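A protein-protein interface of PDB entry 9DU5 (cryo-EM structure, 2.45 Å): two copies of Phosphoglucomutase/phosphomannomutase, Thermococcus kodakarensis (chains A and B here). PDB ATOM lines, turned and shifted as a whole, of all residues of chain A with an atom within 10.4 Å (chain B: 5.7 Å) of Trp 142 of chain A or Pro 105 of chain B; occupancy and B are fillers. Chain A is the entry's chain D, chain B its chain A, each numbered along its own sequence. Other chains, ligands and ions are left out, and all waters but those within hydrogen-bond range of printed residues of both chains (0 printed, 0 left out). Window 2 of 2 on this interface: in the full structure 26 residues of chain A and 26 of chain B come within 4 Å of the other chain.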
ATOM      1  N   ARG A  41      22.734 -21.713   2.355  1.00  0.00           N
ATOM      2  CA  ARG A  41      22.980 -20.868   3.522  1.00  0.00           C
ATOM      3  C   ARG A  41      23.008 -21.766   4.749  1.00  0.00           C
ATOM      4  O   ARG A  41      22.034 -21.825   5.513  1.00  0.00           O
ATOM      5  CB  ARG A  41      21.927 -19.767   3.650  1.00  0.00           C
ATOM      6  CG  ARG A  41      22.311 -18.662   4.619  1.00  0.00           C
ATOM      7  CD  ARG A  41      23.334 -17.723   4.000  1.00  0.00           C
ATOM      8  NE  ARG A  41      23.369 -16.424   4.660  1.00  0.00           N
ATOM      9  CZ  ARG A  41      23.199 -15.264   4.041  1.00  0.00           C
ATOM     10  NH1 ARG A  41      22.986 -15.202   2.737  1.00  0.00           N
ATOM     11  NH2 ARG A  41      23.246 -14.138   4.748  1.00  0.00           N
ATOM     12  N   LEU A  66      31.401 -17.220   9.075  1.00  0.00           N
ATOM     13  CA  LEU A  66      30.653 -16.187   8.367  1.00  0.00           C
ATOM     14  C   LEU A  66      31.275 -15.867   7.014  1.00  0.00           C
ATOM     15  O   LEU A  66      30.552 -15.556   6.062  1.00  0.00           O
ATOM     16  CB  LEU A  66      30.565 -14.920   9.219  1.00  0.00           C
ATOM     17  CG  LEU A  66      29.814 -15.018  10.547  1.00  0.00           C
ATOM     18  CD1 LEU A  66      29.788 -13.671  11.244  1.00  0.00           C
ATOM     19  CD2 LEU A  66      28.408 -15.541  10.340  1.00  0.00           C
ATOM     20  N   SER A  67      32.604 -15.930   6.911  1.00  0.00           N
ATOM     21  CA  SER A  67      33.273 -15.656   5.645  1.00  0.00           C
ATOM     22  C   SER A  67      32.916 -16.667   4.567  1.00  0.00           C
ATOM     23  O   SER A  67      33.026 -16.352   3.379  1.00  0.00           O
ATOM     24  CB  SER A  67      34.787 -15.633   5.847  1.00  0.00           C
ATOM     25  OG  SER A  67      35.285 -16.931   6.109  1.00  0.00           O
ATOM     26  N   THR A  68      32.496 -17.869   4.953  1.00  0.00           N
ATOM     27  CA  THR A  68      32.112 -18.901   4.003  1.00  0.00           C
ATOM     28  C   THR A  68      30.649 -18.822   3.597  1.00  0.00           C
ATOM     29  O   THR A  68      30.215 -19.612   2.753  1.00  0.00           O
ATOM     30  CB  THR A  68      32.397 -20.290   4.586  1.00  0.00           C
ATOM     31  OG1 THR A  68      31.769 -20.408   5.866  1.00  0.00           O
ATOM     32  CG2 THR A  68      33.891 -20.500   4.745  1.00  0.00           C
ATOM     33  N   GLY A  69      29.886 -17.899   4.168  1.00  0.00           N
ATOM     34  CA  GLY A  69      28.484 -17.763   3.851  1.00  0.00           C
ATOM     35  C   GLY A  69      27.536 -18.543   4.732  1.00  0.00           C
ATOM     36  O   GLY A  69      26.372 -18.712   4.354  1.00  0.00           O
ATOM     37  N   HIS A 138      36.007 -21.632   0.648  1.00  0.00           N
ATOM     38  CA  HIS A 138      34.989 -20.910  -0.098  1.00  0.00           C
ATOM     39  C   HIS A 138      34.797 -19.543   0.546  1.00  0.00           C
ATOM     40  O   HIS A 138      34.444 -19.452   1.726  1.00  0.00           O
ATOM     41  CB  HIS A 138      33.672 -21.683  -0.118  1.00  0.00           C
ATOM     42  CG  HIS A 138      32.515 -20.886  -0.635  1.00  0.00           C
ATOM     43  ND1 HIS A 138      32.258 -20.735  -1.980  1.00  0.00           N
ATOM     44  CD2 HIS A 138      31.551 -20.191   0.013  1.00  0.00           C
ATOM     45  CE1 HIS A 138      31.183 -19.985  -2.139  1.00  0.00           C
ATOM     46  NE2 HIS A 138      30.735 -19.641  -0.945  1.00  0.00           N
ATOM     47  N   ARG A 139      35.037 -18.488  -0.222  1.00  0.00           N
ATOM     48  CA  ARG A 139      34.906 -17.122   0.264  1.00  0.00           C
ATOM     49  C   ARG A 139      33.647 -16.519  -0.345  1.00  0.00           C
ATOM     50  O   ARG A 139      33.600 -16.247  -1.548  1.00  0.00           O
ATOM     51  CB  ARG A 139      36.144 -16.302  -0.085  1.00  0.00           C
ATOM     52  CG  ARG A 139      37.425 -16.896   0.463  1.00  0.00           C
ATOM     53  CD  ARG A 139      38.623 -16.003   0.193  1.00  0.00           C
ATOM     54  NE  ARG A 139      39.841 -16.513   0.812  1.00  0.00           N
ATOM     55  CZ  ARG A 139      40.052 -16.590   2.121  1.00  0.00           C
ATOM     56  NH1 ARG A 139      39.150 -16.170   2.995  1.00  0.00           N
ATOM     57  NH2 ARG A 139      41.200 -17.093   2.563  1.00  0.00           N
ATOM     58  N   ALA A 140      32.631 -16.318   0.486  1.00  0.00           N
ATOM     59  CA  ALA A 140      31.376 -15.765   0.012  1.00  0.00           C
ATOM     60  C   ALA A 140      31.558 -14.314  -0.418  1.00  0.00           C
ATOM     61  O   ALA A 140      32.471 -13.612   0.026  1.00  0.00           O
ATOM     62  CB  ALA A 140      30.303 -15.860   1.096  1.00  0.00           C
ATOM     63  N   LYS A 141      30.675 -13.868  -1.307  1.00  0.00           N
ATOM     64  CA  LYS A 141      30.693 -12.484  -1.748  1.00  0.00           C
ATOM     65  C   LYS A 141      30.258 -11.573  -0.604  1.00  0.00           C
ATOM     66  O   LYS A 141      29.818 -12.023   0.457  1.00  0.00           O
ATOM     67  CB  LYS A 141      29.802 -12.305  -2.972  1.00  0.00           C
ATOM     68  CG  LYS A 141      29.991 -13.372  -4.036  1.00  0.00           C
ATOM     69  CD  LYS A 141      31.440 -13.441  -4.492  1.00  0.00           C
ATOM     70  CE  LYS A 141      31.543 -13.453  -6.007  1.00  0.00           C
ATOM     71  NZ  LYS A 141      32.913 -13.096  -6.468  1.00  0.00           N
ATOM     72  N   TRP A 142      30.390 -10.264  -0.824  1.00  0.00           N
ATOM     73  CA  TRP A 142      30.076  -9.304   0.229  1.00  0.00           C
ATOM     74  C   TRP A 142      28.620  -9.409   0.662  1.00  0.00           C
ATOM     75  O   TRP A 142      28.302  -9.234   1.844  1.00  0.00           O
ATOM     76  CB  TRP A 142      30.398  -7.886  -0.242  1.00  0.00           C
ATOM     77  CG  TRP A 142      29.533  -7.420  -1.367  1.00  0.00           C
ATOM     78  CD1 TRP A 142      29.749  -7.608  -2.700  1.00  0.00           C
ATOM     79  CD2 TRP A 142      28.305  -6.693  -1.258  1.00  0.00           C
ATOM     80  NE1 TRP A 142      28.734  -7.040  -3.428  1.00  0.00           N
ATOM     81  CE2 TRP A 142      27.834  -6.472  -2.566  1.00  0.00           C
ATOM     82  CE3 TRP A 142      27.558  -6.207  -0.182  1.00  0.00           C
ATOM     83  CZ2 TRP A 142      26.652  -5.786  -2.826  1.00  0.00           C
ATOM     84  CZ3 TRP A 142      26.386  -5.529  -0.442  1.00  0.00           C
ATOM     85  CH2 TRP A 142      25.944  -5.322  -1.754  1.00  0.00           C
ATOM     86  N   ASN A 143      27.721  -9.700  -0.274  1.00  0.00           N
ATOM     87  CA  ASN A 143      26.301  -9.806   0.026  1.00  0.00           C
ATOM     88  C   ASN A 143      25.884 -11.206   0.456  1.00  0.00           C
ATOM     89  O   ASN A 143      24.741 -11.389   0.885  1.00  0.00           O
ATOM     90  CB  ASN A 143      25.474  -9.371  -1.188  1.00  0.00           C
ATOM     91  CG  ASN A 143      25.757 -10.209  -2.416  1.00  0.00           C
ATOM     92  OD1 ASN A 143      26.903 -10.334  -2.845  1.00  0.00           O
ATOM     93  ND2 ASN A 143      24.710 -10.788  -2.990  1.00  0.00           N
ATOM     94  N   GLU A 144      26.774 -12.192   0.357  1.00  0.00           N
ATOM     95  CA  GLU A 144      26.473 -13.560   0.754  1.00  0.00           C
ATOM     96  C   GLU A 144      27.093 -13.934   2.092  1.00  0.00           C
ATOM     97  O   GLU A 144      27.008 -15.097   2.499  1.00  0.00           O
ATOM     98  CB  GLU A 144      26.937 -14.539  -0.324  1.00  0.00           C
ATOM     99  CG  GLU A 144      26.262 -14.352  -1.667  1.00  0.00           C
ATOM    100  CD  GLU A 144      27.020 -15.029  -2.788  1.00  0.00           C
ATOM    101  OE1 GLU A 144      27.877 -15.887  -2.489  1.00  0.00           O
ATOM    102  OE2 GLU A 144      26.760 -14.705  -3.965  1.00  0.00           O
ATOM    103  N   ILE A 145      27.719 -12.982   2.784  1.00  0.00           N
ATOM    104  CA  ILE A 145      28.341 -13.277   4.065  1.00  0.00           C
ATOM    105  C   ILE A 145      27.265 -13.571   5.103  1.00  0.00           C
ATOM    106  O   ILE A 145      26.262 -12.853   5.218  1.00  0.00           O
ATOM    107  CB  ILE A 145      29.249 -12.111   4.498  1.00  0.00           C
ATOM    108  CG1 ILE A 145      30.545 -12.136   3.687  1.00  0.00           C
ATOM    109  CG2 ILE A 145      29.555 -12.180   5.983  1.00  0.00           C
ATOM    110  CD1 ILE A 145      31.384 -10.900   3.839  1.00  0.00           C
ATOM    111  N   GLY A 146      27.469 -14.646   5.863  1.00  0.00           N
ATOM    112  CA  GLY A 146      26.446 -15.119   6.769  1.00  0.00           C
ATOM    113  C   GLY A 146      26.183 -14.166   7.919  1.00  0.00           C
ATOM    114  O   GLY A 146      27.000 -13.316   8.274  1.00  0.00           O
ATOM    115  N   GLU A 147      25.004 -14.324   8.510  1.00  0.00           N
ATOM    116  CA  GLU A 147      24.564 -13.512   9.632  1.00  0.00           C
ATOM    117  C   GLU A 147      24.777 -14.263  10.941  1.00  0.00           C
ATOM    118  O   GLU A 147      24.769 -15.495  10.981  1.00  0.00           O
ATOM    119  CB  GLU A 147      23.090 -13.133   9.486  1.00  0.00           C
ATOM    120  CG  GLU A 147      22.859 -11.811   8.780  1.00  0.00           C
ATOM    121  CD  GLU A 147      22.645 -11.979   7.290  1.00  0.00           C
ATOM    122  OE1 GLU A 147      21.972 -12.953   6.894  1.00  0.00           O
ATOM    123  OE2 GLU A 147      23.150 -11.139   6.516  1.00  0.00           O
ATOM    124  N   ALA B  14      36.070  -6.670   0.465  1.00  0.00           N
ATOM    125  CA  ALA B  14      35.814  -7.595   1.559  1.00  0.00           C
ATOM    126  C   ALA B  14      35.804  -9.035   1.065  1.00  0.00           C
ATOM    127  O   ALA B  14      35.303  -9.333  -0.023  1.00  0.00           O
ATOM    128  CB  ALA B  14      34.485  -7.261   2.230  1.00  0.00           C
ATOM    129  N   ASN B  15      36.377  -9.926   1.873  1.00  0.00           N
ATOM    130  CA  ASN B  15      36.471 -11.362   1.622  1.00  0.00           C
ATOM    131  C   ASN B  15      37.353 -11.703   0.426  1.00  0.00           C
ATOM    132  O   ASN B  15      37.496 -12.882   0.087  1.00  0.00           O
ATOM    133  CB  ASN B  15      35.085 -11.997   1.448  1.00  0.00           C
ATOM    134  CG  ASN B  15      34.862 -13.165   2.383  1.00  0.00           C
ATOM    135  OD1 ASN B  15      35.750 -13.544   3.145  1.00  0.00           O
ATOM    136  ND2 ASN B  15      33.669 -13.743   2.333  1.00  0.00           N
ATOM    137  N   ARG B  51      28.307  -1.827   7.301  1.00  0.00           N
ATOM    138  CA  ARG B  51      28.639  -2.720   6.200  1.00  0.00           C
ATOM    139  C   ARG B  51      28.437  -4.181   6.595  1.00  0.00           C
ATOM    140  O   ARG B  51      28.731  -4.599   7.717  1.00  0.00           O
ATOM    141  CB  ARG B  51      30.080  -2.496   5.746  1.00  0.00           C
ATOM    142  CG  ARG B  51      30.272  -1.233   4.932  1.00  0.00           C
ATOM    143  CD  ARG B  51      31.741  -0.923   4.724  1.00  0.00           C
ATOM    144  NE  ARG B  51      31.929   0.414   4.174  1.00  0.00           N
ATOM    145  CZ  ARG B  51      31.801   0.723   2.892  1.00  0.00           C
ATOM    146  NH1 ARG B  51      31.504  -0.194   1.987  1.00  0.00           N
ATOM    147  NH2 ARG B  51      31.973   1.983   2.509  1.00  0.00           N
ATOM    148  N   VAL B  52      27.921  -4.960   5.643  1.00  0.00           N
ATOM    149  CA  VAL B  52      27.548  -6.344   5.916  1.00  0.00           C
ATOM    150  C   VAL B  52      28.745  -7.219   6.256  1.00  0.00           C
ATOM    151  O   VAL B  52      28.596  -8.194   7.004  1.00  0.00           O
ATOM    152  CB  VAL B  52      26.785  -6.941   4.722  1.00  0.00           C
ATOM    153  CG1 VAL B  52      25.338  -6.486   4.745  1.00  0.00           C
ATOM    154  CG2 VAL B  52      27.445  -6.536   3.421  1.00  0.00           C
ATOM    155  N   SER B  53      29.926  -6.906   5.733  1.00  0.00           N
ATOM    156  CA  SER B  53      31.132  -7.659   6.039  1.00  0.00           C
ATOM    157  C   SER B  53      31.803  -7.202   7.326  1.00  0.00           C
ATOM    158  O   SER B  53      32.819  -7.781   7.718  1.00  0.00           O
ATOM    159  CB  SER B  53      32.124  -7.550   4.882  1.00  0.00           C
ATOM    160  OG  SER B  53      32.386  -6.194   4.567  1.00  0.00           O
ATOM    161  N   ASN B 103      33.376   4.059   0.296  1.00  0.00           N
ATOM    162  CA  ASN B 103      33.581   3.095  -0.768  1.00  0.00           C
ATOM    163  C   ASN B 103      32.317   2.269  -1.003  1.00  0.00           C
ATOM    164  O   ASN B 103      31.448   2.185  -0.133  1.00  0.00           O
ATOM    165  CB  ASN B 103      34.761   2.192  -0.427  1.00  0.00           C
ATOM    166  CG  ASN B 103      36.091   2.868  -0.669  1.00  0.00           C
ATOM    167  OD1 ASN B 103      36.416   3.869  -0.032  1.00  0.00           O
ATOM    168  ND2 ASN B 103      36.870   2.327  -1.597  1.00  0.00           N
ATOM    169  N   PRO B 104      32.188   1.661  -2.182  1.00  0.00           N
ATOM    170  CA  PRO B 104      30.992   0.864  -2.497  1.00  0.00           C
ATOM    171  C   PRO B 104      30.794  -0.269  -1.503  1.00  0.00           C
ATOM    172  O   PRO B 104      31.698  -0.577  -0.712  1.00  0.00           O
ATOM    173  CB  PRO B 104      31.298   0.333  -3.906  1.00  0.00           C
ATOM    174  CG  PRO B 104      32.195   1.356  -4.485  1.00  0.00           C
ATOM    175  CD  PRO B 104      33.073   1.787  -3.354  1.00  0.00           C
ATOM    176  N   PRO B 105      29.622  -0.916  -1.515  1.00  0.00           N
ATOM    177  CA  PRO B 105      29.313  -1.907  -0.470  1.00  0.00           C
ATOM    178  C   PRO B 105      30.276  -3.081  -0.400  1.00  0.00           C
ATOM    179  O   PRO B 105      30.402  -3.682   0.673  1.00  0.00           O
ATOM    180  CB  PRO B 105      27.905  -2.378  -0.856  1.00  0.00           C
ATOM    181  CG  PRO B 105      27.329  -1.198  -1.552  1.00  0.00           C
ATOM    182  CD  PRO B 105      28.465  -0.721  -2.403  1.00  0.00           C
ATOM    183  N   GLU B 106      30.948  -3.432  -1.492  1.00  0.00           N
ATOM    184  CA  GLU B 106      31.836  -4.585  -1.514  1.00  0.00           C
ATOM    185  C   GLU B 106      33.160  -4.333  -0.808  1.00  0.00           C
ATOM    186  O   GLU B 106      33.943  -5.273  -0.638  1.00  0.00           O
ATOM    187  CB  GLU B 106      32.103  -5.020  -2.958  1.00  0.00           C
ATOM    188  CG  GLU B 106      32.446  -3.882  -3.901  1.00  0.00           C
ATOM    189  CD  GLU B 106      31.232  -3.338  -4.625  1.00  0.00           C
ATOM    190  OE1 GLU B 106      30.106  -3.778  -4.314  1.00  0.00           O
ATOM    191  OE2 GLU B 106      31.405  -2.474  -5.509  1.00  0.00           O
ATOM    192  N   TYR B 107      33.433  -3.101  -0.396  1.00  0.00           N
ATOM    193  CA  TYR B 107      34.693  -2.751   0.238  1.00  0.00           C
ATOM    194  C   TYR B 107      34.558  -2.724   1.754  1.00  0.00           C
ATOM    195  O   TYR B 107      33.469  -2.555   2.307  1.00  0.00           O
ATOM    196  CB  TYR B 107      35.196  -1.392  -0.255  1.00  0.00           C
ATOM    197  CG  TYR B 107      35.763  -1.407  -1.653  1.00  0.00           C
ATOM    198  CD1 TYR B 107      34.959  -1.683  -2.748  1.00  0.00           C
ATOM    199  CD2 TYR B 107      37.107  -1.152  -1.876  1.00  0.00           C
ATOM    200  CE1 TYR B 107      35.476  -1.700  -4.025  1.00  0.00           C
ATOM    201  CE2 TYR B 107      37.634  -1.166  -3.149  1.00  0.00           C
ATOM    202  CZ  TYR B 107      36.814  -1.441  -4.220  1.00  0.00           C
ATOM    203  OH  TYR B 107      37.332  -1.457  -5.494  1.00  0.00           O
ATOM    204  N   ASN B 108      35.694  -2.898   2.419  1.00  0.00           N
ATOM    205  CA  ASN B 108      35.789  -2.757   3.865  1.00  0.00           C
ATOM    206  C   ASN B 108      37.248  -2.500   4.207  1.00  0.00           C
ATOM    207  O   ASN B 108      38.134  -2.615   3.358  1.00  0.00           O
ATOM    208  CB  ASN B 108      35.249  -3.990   4.592  1.00  0.00           C
ATOM    209  CG  ASN B 108      34.446  -3.631   5.825  1.00  0.00           C
ATOM    210  OD1 ASN B 108      34.735  -2.647   6.501  1.00  0.00           O
ATOM    211  ND2 ASN B 108      33.425  -4.424   6.120  1.00  0.00           N
ATOM    212  N   GLY B 210      23.718  -2.351   5.375  1.00  0.00           N
ATOM    213  CA  GLY B 210      25.029  -2.490   4.785  1.00  0.00           C
ATOM    214  C   GLY B 210      25.042  -2.793   3.306  1.00  0.00           C
ATOM    215  O   GLY B 210      26.111  -2.757   2.689  1.00  0.00           O
ATOM    216  N   HIS B 211      23.890  -3.097   2.716  1.00  0.00           N
ATOM    217  CA  HIS B 211      23.789  -3.298   1.281  1.00  0.00           C
ATOM    218  C   HIS B 211      23.667  -1.990   0.515  1.00  0.00           C
ATOM    219  O   HIS B 211      23.869  -1.985  -0.704  1.00  0.00           O
ATOM    220  CB  HIS B 211      22.589  -4.190   0.956  1.00  0.00           C
ATOM    221  CG  HIS B 211      22.758  -5.611   1.393  1.00  0.00           C
ATOM    222  ND1 HIS B 211      23.224  -6.599   0.553  1.00  0.00           N
ATOM    223  CD2 HIS B 211      22.524  -6.210   2.584  1.00  0.00           C
ATOM    224  CE1 HIS B 211      23.270  -7.746   1.207  1.00  0.00           C
ATOM    225  NE2 HIS B 211      22.850  -7.537   2.442  1.00  0.00           N
ATOM    226  N   PHE B 212      23.355  -0.889   1.204  1.00  0.00           N
ATOM    227  CA  PHE B 212      23.166   0.432   0.619  1.00  0.00           C
ATOM    228  C   PHE B 212      22.206   0.355  -0.563  1.00  0.00           C
ATOM    229  O   PHE B 212      22.617   0.565  -1.711  1.00  0.00           O
ATOM    230  CB  PHE B 212      24.514   1.022   0.202  1.00  0.00           C
ATOM    231  CG  PHE B 212      25.485   1.166   1.340  1.00  0.00           C
ATOM    232  CD1 PHE B 212      25.186   1.970   2.425  1.00  0.00           C
ATOM    233  CD2 PHE B 212      26.688   0.482   1.335  1.00  0.00           C
ATOM    234  CE1 PHE B 212      26.074   2.098   3.474  1.00  0.00           C
ATOM    235  CE2 PHE B 212      27.577   0.605   2.381  1.00  0.00           C
ATOM    236  CZ  PHE B 212      27.269   1.414   3.452  1.00  0.00           C
ATOM    237  N   ASN B 216      25.472   4.484  -3.550  1.00  0.00           N
ATOM    238  CA  ASN B 216      26.759   4.328  -2.897  1.00  0.00           C
ATOM    239  C   ASN B 216      26.889   5.357  -1.775  1.00  0.00           C
ATOM    240  O   ASN B 216      26.376   6.474  -1.894  1.00  0.00           O
ATOM    241  CB  ASN B 216      27.897   4.493  -3.901  1.00  0.00           C
ATOM    242  CG  ASN B 216      28.195   3.212  -4.655  1.00  0.00           C
ATOM    243  OD1 ASN B 216      27.614   2.164  -4.375  1.00  0.00           O
ATOM    244  ND2 ASN B 216      29.102   3.291  -5.621  1.00  0.00           N
ATOM    245  N   PRO B 217      27.563   5.016  -0.679  1.00  0.00           N
ATOM    246  CA  PRO B 217      27.573   5.910   0.487  1.00  0.00           C
ATOM    247  C   PRO B 217      28.351   7.202   0.285  1.00  0.00           C
ATOM    248  O   PRO B 217      28.502   7.975   1.234  1.00  0.00           O
ATOM    249  CB  PRO B 217      28.215   5.041   1.578  1.00  0.00           C
ATOM    250  CG  PRO B 217      29.033   4.056   0.819  1.00  0.00           C
ATOM    251  CD  PRO B 217      28.190   3.721  -0.368  1.00  0.00           C
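Of the 15 printed residues of chain A, 6 touch a printed residue of chain B.
Among the printed residues, no Asp or Glu carboxylate lies within 4 Å of a Lys or Arg side-chain nitrogen of the other chain.
N of Ala 140 of chain A is in hydrogen-bond range of O of Ser 67 of chain A, 2.9 Å away.
The side-chain hydroxyl of Ser 53 of chain B is in hydrogen-bond range of the side-chain amide nitrogen of Asn 108 of chain B (2.6 Å).
O of Glu 106 of chain B is in hydrogen-bond range of N of Ala 14 of chain B (2.8 Å).
The guanidinium group of Arg 41 of chain A sits at hydrogen-bond distance from the backbone carbonyl oxygen of Ile 145 of chain A.
No position is printed for both chains.
Of the 10 pairs that touch across the chains among the printed residues, none has its exchanged pair printed and touching as well.
Trp 142 of chain A touches just these residues of chain B: Val 52 (3.2 Å), Pro 105 (3.5 Å), Glu 106 (3.5 Å) and His 211 (3.5 Å).
Pro 105 of chain B touches just one residue of chain A: Trp 142 (3.5 Å).
No residue of chain A comes within 4 Å of Ala 14 of chain B.
Of chain A, only Trp 142 comes within 4 Å of Val 52 of chain B.
No residue of chain A comes within 4 Å of Pro 104 of chain B.
His 211 of chain B touches just these residues of chain A: Trp 142 and Asn 143.
No residue of chain A comes within 4 Å of Phe 212 of chain B.
Printed residues of chain B within 4 Å of Asn 143 of chain A: His 211.
Printed residues of chain A within 4 Å of Ser 53 of chain B: Ile 145 (3.6 Å).
Of the printed residues of chain B, Arg 139 of chain A touches Asn 15 (3.3 Å).
Printed residues of chain B within 4 Å of Ile 145 of chain A: Asn 15 and Ser 53.
The nearest residue of chain A that does not touch Pro 105 of chain B is Asn 143 of chain A (6.7 Å).
ND2 of Asn 15 of chain B sits at hydrogen-bond distance from O of Ser 67 of chain A, at 2.9 Å.
O of Ala 140 of chain A is in hydrogen-bond range of ND2 of Asn 15 of chain B, at 2.6 Å.
Among the printed residues, merely in contact across the chains: Arg 139 of chain A with Asn 15 of chain B, Trp 142 of chain A with Val 52 of chain B, Trp 142 of chain A with Pro 105 of chain B, Trp 142 of chain A with Glu 106 of chain B, Trp 142 of chain A with His 211 of chain B, Asn 143 of chain A with His 211 of chain B, Ile 145 of chain A with Asn 15 of chain B and Ile 145 of chain A with Ser 53 of chain B.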
